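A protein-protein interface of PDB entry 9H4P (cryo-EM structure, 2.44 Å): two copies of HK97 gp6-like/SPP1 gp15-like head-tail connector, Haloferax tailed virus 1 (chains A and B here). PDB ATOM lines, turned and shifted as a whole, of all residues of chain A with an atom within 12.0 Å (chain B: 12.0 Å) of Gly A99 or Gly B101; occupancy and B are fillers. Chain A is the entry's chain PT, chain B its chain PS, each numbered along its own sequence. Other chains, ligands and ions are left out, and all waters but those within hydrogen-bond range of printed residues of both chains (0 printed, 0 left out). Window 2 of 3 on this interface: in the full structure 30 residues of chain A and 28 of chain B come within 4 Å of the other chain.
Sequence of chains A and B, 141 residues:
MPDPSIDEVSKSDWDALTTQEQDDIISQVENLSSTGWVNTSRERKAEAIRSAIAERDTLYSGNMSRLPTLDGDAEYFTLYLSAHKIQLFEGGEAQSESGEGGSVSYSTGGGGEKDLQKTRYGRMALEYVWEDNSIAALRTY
O of Ser B103 is in hydrogen-bond range of N of Ser A98 (2.9 Å). The backbone carbonyl oxygen (O) of Ser A96 is in hydrogen-bond range of the backbone NH (N) of Ser B105 (3.0 Å). The backbone carbonyl oxygen (O) of Ser B105 lies within hydrogen-bond range of the backbone NH (N) of Gln A95, at 2.7 Å.
The backbone carbonyl oxygen (O) of Val A104 lies within hydrogen-bond range of the side-chain hydroxyl (OG) of Ser A96 (2.6 Å). OG of Ser B98 lies within hydrogen-bond range of OG of Ser B103. N of Val B104 sits at hydrogen-bond distance from O of Glu B97 (2.9 Å). OG of Ser A98 sits at hydrogen-bond distance from OG of Ser A103, at 2.7 Å. The backbone carbonyl oxygen of Gln A95 lies within hydrogen-bond range of the backbone NH of Tyr A106 (2.8 Å). O of Gln A95 lies close to OG of Ser A105 (3.4 Å).
Ser A96 touches Val B104, but with the chains exchanged Val A104 does not touch Ser B96 (10.5 Å). Ser A96 touches Ser B105, but with the chains exchanged Ser A105 does not touch Ser B96 (11.4 Å). Ser A98 touches Gly B102, but with the chains exchanged Gly A102 does not touch Ser B98 (11.3 Å). Gly A99 touches Gly B101, but with the chains exchanged Gly A101 does not touch Gly B99 (11.2 Å). 10 positions are printed for both chains.
Printed residues of chain A that touch a printed residue of chain B: Ala A94, Gln A95, Ser A96, Glu A97, Ser A98 and Gly A99. Of the 10 printed residues of chain B, 5 touch a printed residue of chain A. Among the printed residues, no Asp or Glu carboxylate lies within 4 Å of a Lys or Arg side-chain nitrogen of the other chain.
Among the printed residues, merely in contact across the chains: Ala A94 with Ser B105, Ser A96 with Val B104, Glu A97 with Ser B103, Ser A98 with Gly B102 and Gly A99 with Gly B101.
Ser A98 touches just these residues of chain B: Gly B102 and Ser B103. Glu A100 touches none of the printed residues of chain B. No residue of chain B comes within 4 Å of Gly A101. No residue of chain B comes within 4 Å of Ser A103. No residue of chain A comes within 4 Å of Ser B98. Glu B100 touches none of the printed residues of chain A. Gly B102 touches just one residue of chain A: Ser A98 (3.5 Å). Printed residues of chain B within 4 Å of Gln A95: Ser B105. Printed residues of chain B within 4 Å of Ala A94: Ser B105 (3.4 Å). Glu B97 touches none of the printed residues of chain A. Ser A105 touches none of the printed residues of chain B. The nearest residue of chain B that does not touch Gly A99 is Gly B102 (4.5 Å). The nearest residue of chain A that does not touch Gly B101 is Ser A98 (4.1 Å).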
ATOM      1  N   ALA A  94      25.330  34.517  25.483  1.00  0.00           N
ATOM      2  CA  ALA A  94      25.178  33.071  25.480  1.00  0.00           C
ATOM      3  C   ALA A  94      25.568  32.531  26.857  1.00  0.00           C
ATOM      4  O   ALA A  94      26.722  32.653  27.262  1.00  0.00           O
ATOM      5  CB  ALA A  94      26.000  32.453  24.374  1.00  0.00           C
ATOM      6  N   GLN A  95      24.586  31.970  27.582  1.00  0.00           N
ATOM      7  CA  GLN A  95      24.814  31.255  28.834  1.00  0.00           C
ATOM      8  C   GLN A  95      25.455  29.900  28.531  1.00  0.00           C
ATOM      9  O   GLN A  95      26.325  29.453  29.275  1.00  0.00           O
ATOM     10  CB  GLN A  95      23.509  31.111  29.630  1.00  0.00           C
ATOM     11  CG  GLN A  95      23.606  30.263  30.897  1.00  0.00           C
ATOM     12  CD  GLN A  95      22.318  30.164  31.677  1.00  0.00           C
ATOM     13  OE1 GLN A  95      21.328  30.827  31.383  1.00  0.00           O
ATOM     14  NE2 GLN A  95      22.321  29.322  32.693  1.00  0.00           N
ATOM     15  N   SER A  96      25.018  29.255  27.436  1.00  0.00           N
ATOM     16  CA  SER A  96      25.540  27.963  27.007  1.00  0.00           C
ATOM     17  C   SER A  96      25.393  27.790  25.493  1.00  0.00           C
ATOM     18  O   SER A  96      24.464  28.328  24.893  1.00  0.00           O
ATOM     19  CB  SER A  96      24.879  26.829  27.762  1.00  0.00           C
ATOM     20  OG  SER A  96      25.357  25.565  27.325  1.00  0.00           O
ATOM     21  N   GLU A  97      26.331  27.037  24.894  1.00  0.00           N
ATOM     22  CA  GLU A  97      26.330  26.657  23.484  1.00  0.00           C
ATOM     23  C   GLU A  97      26.616  25.155  23.374  1.00  0.00           C
ATOM     24  O   GLU A  97      27.368  24.622  24.188  1.00  0.00           O
ATOM     25  CB  GLU A  97      27.401  27.438  22.712  1.00  0.00           C
ATOM     26  CG  GLU A  97      27.205  28.947  22.691  1.00  0.00           C
ATOM     27  CD  GLU A  97      28.367  29.712  22.089  1.00  0.00           C
ATOM     28  OE1 GLU A  97      29.475  29.636  22.647  1.00  0.00           O
ATOM     29  OE2 GLU A  97      28.161  30.374  21.060  1.00  0.00           O
ATOM     30  N   SER A  98      26.031  24.484  22.363  1.00  0.00           N
ATOM     31  CA  SER A  98      26.176  23.042  22.161  1.00  0.00           C
ATOM     32  C   SER A  98      26.024  22.658  20.682  1.00  0.00           C
ATOM     33  O   SER A  98      25.272  23.301  19.951  1.00  0.00           O
ATOM     34  CB  SER A  98      25.201  22.277  23.035  1.00  0.00           C
ATOM     35  OG  SER A  98      25.424  20.875  22.962  1.00  0.00           O
ATOM     36  N   GLY A  99      26.730  21.592  20.256  1.00  0.00           N
ATOM     37  CA  GLY A  99      26.680  21.046  18.900  1.00  0.00           C
ATOM     38  C   GLY A  99      27.758  19.982  18.664  1.00  0.00           C
ATOM     39  O   GLY A  99      28.335  19.478  19.629  1.00  0.00           O
ATOM     40  N   GLU A 100      28.055  19.668  17.387  1.00  0.00           N
ATOM     41  CA  GLU A 100      29.080  18.688  17.030  1.00  0.00           C
ATOM     42  C   GLU A 100      30.503  19.209  17.274  1.00  0.00           C
ATOM     43  O   GLU A 100      31.461  18.442  17.179  1.00  0.00           O
ATOM     44  CB  GLU A 100      28.891  18.162  15.605  1.00  0.00           C
ATOM     45  CG  GLU A 100      27.613  17.369  15.398  1.00  0.00           C
ATOM     46  CD  GLU A 100      27.370  16.193  16.327  1.00  0.00           C
ATOM     47  OE1 GLU A 100      28.335  15.494  16.672  1.00  0.00           O
ATOM     48  OE2 GLU A 100      26.209  15.980  16.699  1.00  0.00           O
ATOM     49  N   GLY A 101      30.638  20.500  17.603  1.00  0.00           N
ATOM     50  CA  GLY A 101      31.881  21.039  18.137  1.00  0.00           C
ATOM     51  C   GLY A 101      32.126  20.662  19.601  1.00  0.00           C
ATOM     52  O   GLY A 101      33.247  20.801  20.089  1.00  0.00           O
ATOM     53  N   GLY A 102      31.075  20.178  20.287  1.00  0.00           N
ATOM     54  CA  GLY A 102      31.061  19.952  21.729  1.00  0.00           C
ATOM     55  C   GLY A 102      30.157  20.956  22.450  1.00  0.00           C
ATOM     56  O   GLY A 102      29.315  21.579  21.808  1.00  0.00           O
ATOM     57  N   SER A 103      30.336  21.124  23.774  1.00  0.00           N
ATOM     58  CA  SER A 103      29.461  21.970  24.587  1.00  0.00           C
ATOM     59  C   SER A 103      30.238  22.830  25.591  1.00  0.00           C
ATOM     60  O   SER A 103      31.334  22.459  26.010  1.00  0.00           O
ATOM     61  CB  SER A 103      28.403  21.150  25.287  1.00  0.00           C
ATOM     62  OG  SER A 103      27.657  20.371  24.364  1.00  0.00           O
ATOM     63  N   VAL A 104      29.642  23.968  25.988  1.00  0.00           N
ATOM     64  CA  VAL A 104      30.226  24.930  26.921  1.00  0.00           C
ATOM     65  C   VAL A 104      29.112  25.633  27.710  1.00  0.00           C
ATOM     66  O   VAL A 104      27.993  25.758  27.214  1.00  0.00           O
ATOM     67  CB  VAL A 104      31.164  25.928  26.198  1.00  0.00           C
ATOM     68  CG1 VAL A 104      30.482  26.684  25.062  1.00  0.00           C
ATOM     69  CG2 VAL A 104      31.874  26.890  27.146  1.00  0.00           C
ATOM     70  N   SER A 105      29.423  26.069  28.941  1.00  0.00           N
ATOM     71  CA  SER A 105      28.569  26.941  29.740  1.00  0.00           C
ATOM     72  C   SER A 105      29.418  28.049  30.368  1.00  0.00           C
ATOM     73  O   SER A 105      30.538  27.786  30.800  1.00  0.00           O
ATOM     74  CB  SER A 105      27.802  26.155  30.780  1.00  0.00           C
ATOM     75  OG  SER A 105      26.994  27.007  31.581  1.00  0.00           O
ATOM     76  N   TYR A 106      28.878  29.279  30.429  1.00  0.00           N
ATOM     77  CA  TYR A 106      29.679  30.479  30.656  1.00  0.00           C
ATOM     78  C   TYR A 106      29.404  31.184  31.995  1.00  0.00           C
ATOM     79  O   TYR A 106      29.574  32.400  32.078  1.00  0.00           O
ATOM     80  CB  TYR A 106      29.503  31.462  29.494  1.00  0.00           C
ATOM     81  CG  TYR A 106      30.039  31.037  28.148  1.00  0.00           C
ATOM     82  CD1 TYR A 106      31.388  31.143  27.846  1.00  0.00           C
ATOM     83  CD2 TYR A 106      29.184  30.597  27.147  1.00  0.00           C
ATOM     84  CE1 TYR A 106      31.876  30.795  26.598  1.00  0.00           C
ATOM     85  CE2 TYR A 106      29.654  30.247  25.892  1.00  0.00           C
ATOM     86  CZ  TYR A 106      31.005  30.351  25.619  1.00  0.00           C
ATOM     87  OH  TYR A 106      31.487  30.000  24.396  1.00  0.00           O
ATOM     88  N   SER B  96      16.033  29.964  25.292  1.00  0.00           N
ATOM     89  CA  SER B  96      16.848  28.954  24.632  1.00  0.00           C
ATOM     90  C   SER B  96      16.260  28.598  23.266  1.00  0.00           C
ATOM     91  O   SER B  96      15.045  28.639  23.082  1.00  0.00           O
ATOM     92  CB  SER B  96      17.006  27.730  25.507  1.00  0.00           C
ATOM     93  OG  SER B  96      17.779  26.728  24.861  1.00  0.00           O
ATOM     94  N   GLU B  97      17.146  28.247  22.319  1.00  0.00           N
ATOM     95  CA  GLU B  97      16.803  27.812  20.969  1.00  0.00           C
ATOM     96  C   GLU B  97      17.630  26.575  20.617  1.00  0.00           C
ATOM     97  O   GLU B  97      18.815  26.520  20.940  1.00  0.00           O
ATOM     98  CB  GLU B  97      17.056  28.942  19.965  1.00  0.00           C
ATOM     99  CG  GLU B  97      16.087  30.102  20.105  1.00  0.00           C
ATOM    100  CD  GLU B  97      16.300  31.263  19.155  1.00  0.00           C
ATOM    101  OE1 GLU B  97      17.430  31.775  19.083  1.00  0.00           O
ATOM    102  OE2 GLU B  97      15.332  31.654  18.492  1.00  0.00           O
ATOM    103  N   SER B  98      17.001  25.595  19.948  1.00  0.00           N
ATOM    104  CA  SER B  98      17.623  24.316  19.621  1.00  0.00           C
ATOM    105  C   SER B  98      17.042  23.745  18.325  1.00  0.00           C
ATOM    106  O   SER B  98      15.851  23.909  18.066  1.00  0.00           O
ATOM    107  CB  SER B  98      17.459  23.344  20.767  1.00  0.00           C
ATOM    108  OG  SER B  98      18.109  22.109  20.501  1.00  0.00           O
ATOM    109  N   GLY B  99      17.877  23.062  17.525  1.00  0.00           N
ATOM    110  CA  GLY B  99      17.459  22.446  16.270  1.00  0.00           C
ATOM    111  C   GLY B  99      18.614  21.733  15.564  1.00  0.00           C
ATOM    112  O   GLY B  99      19.741  22.227  15.585  1.00  0.00           O
ATOM    113  N   GLU B 100      18.325  20.556  14.980  1.00  0.00           N
ATOM    114  CA  GLU B 100      19.278  19.708  14.266  1.00  0.00           C
ATOM    115  C   GLU B 100      20.524  19.392  15.105  1.00  0.00           C
ATOM    116  O   GLU B 100      21.616  19.223  14.558  1.00  0.00           O
ATOM    117  CB  GLU B 100      19.583  20.287  12.877  1.00  0.00           C
ATOM    118  CG  GLU B 100      18.415  20.199  11.913  1.00  0.00           C
ATOM    119  CD  GLU B 100      17.891  18.789  11.725  1.00  0.00           C
ATOM    120  OE1 GLU B 100      18.616  17.964  11.150  1.00  0.00           O
ATOM    121  OE2 GLU B 100      16.770  18.515  12.186  1.00  0.00           O
ATOM    122  N   GLY B 101      20.348  19.297  16.431  1.00  0.00           N
ATOM    123  CA  GLY B 101      21.428  18.989  17.359  1.00  0.00           C
ATOM    124  C   GLY B 101      22.170  20.214  17.901  1.00  0.00           C
ATOM    125  O   GLY B 101      22.812  20.114  18.945  1.00  0.00           O
ATOM    126  N   GLY B 102      22.099  21.355  17.199  1.00  0.00           N
ATOM    127  CA  GLY B 102      22.656  22.605  17.700  1.00  0.00           C
ATOM    128  C   GLY B 102      21.748  23.238  18.756  1.00  0.00           C
ATOM    129  O   GLY B 102      20.530  23.168  18.624  1.00  0.00           O
ATOM    130  N   SER B 103      22.339  23.850  19.801  1.00  0.00           N
ATOM    131  CA  SER B 103      21.584  24.482  20.884  1.00  0.00           C
ATOM    132  C   SER B 103      22.304  25.707  21.458  1.00  0.00           C
ATOM    133  O   SER B 103      23.534  25.757  21.459  1.00  0.00           O
ATOM    134  CB  SER B 103      21.265  23.502  21.996  1.00  0.00           C
ATOM    135  OG  SER B 103      20.583  22.355  21.512  1.00  0.00           O
ATOM    136  N   VAL B 104      21.519  26.663  21.993  1.00  0.00           N
ATOM    137  CA  VAL B 104      22.010  27.859  22.674  1.00  0.00           C
ATOM    138  C   VAL B 104      21.021  28.287  23.769  1.00  0.00           C
ATOM    139  O   VAL B 104      19.827  28.010  23.664  1.00  0.00           O
ATOM    140  CB  VAL B 104      22.327  28.998  21.675  1.00  0.00           C
ATOM    141  CG1 VAL B 104      21.125  29.416  20.836  1.00  0.00           C
ATOM    142  CG2 VAL B 104      22.993  30.212  22.319  1.00  0.00           C
ATOM    143  N   SER B 105      21.535  28.957  24.817  1.00  0.00           N
ATOM    144  CA  SER B 105      20.756  29.551  25.898  1.00  0.00           C
ATOM    145  C   SER B 105      21.245  30.981  26.147  1.00  0.00           C
ATOM    146  O   SER B 105      22.451  31.216  26.113  1.00  0.00           O
ATOM    147  CB  SER B 105      20.848  28.698  27.143  1.00  0.00           C
ATOM    148  OG  SER B 105      20.115  29.267  28.218  1.00  0.00           O
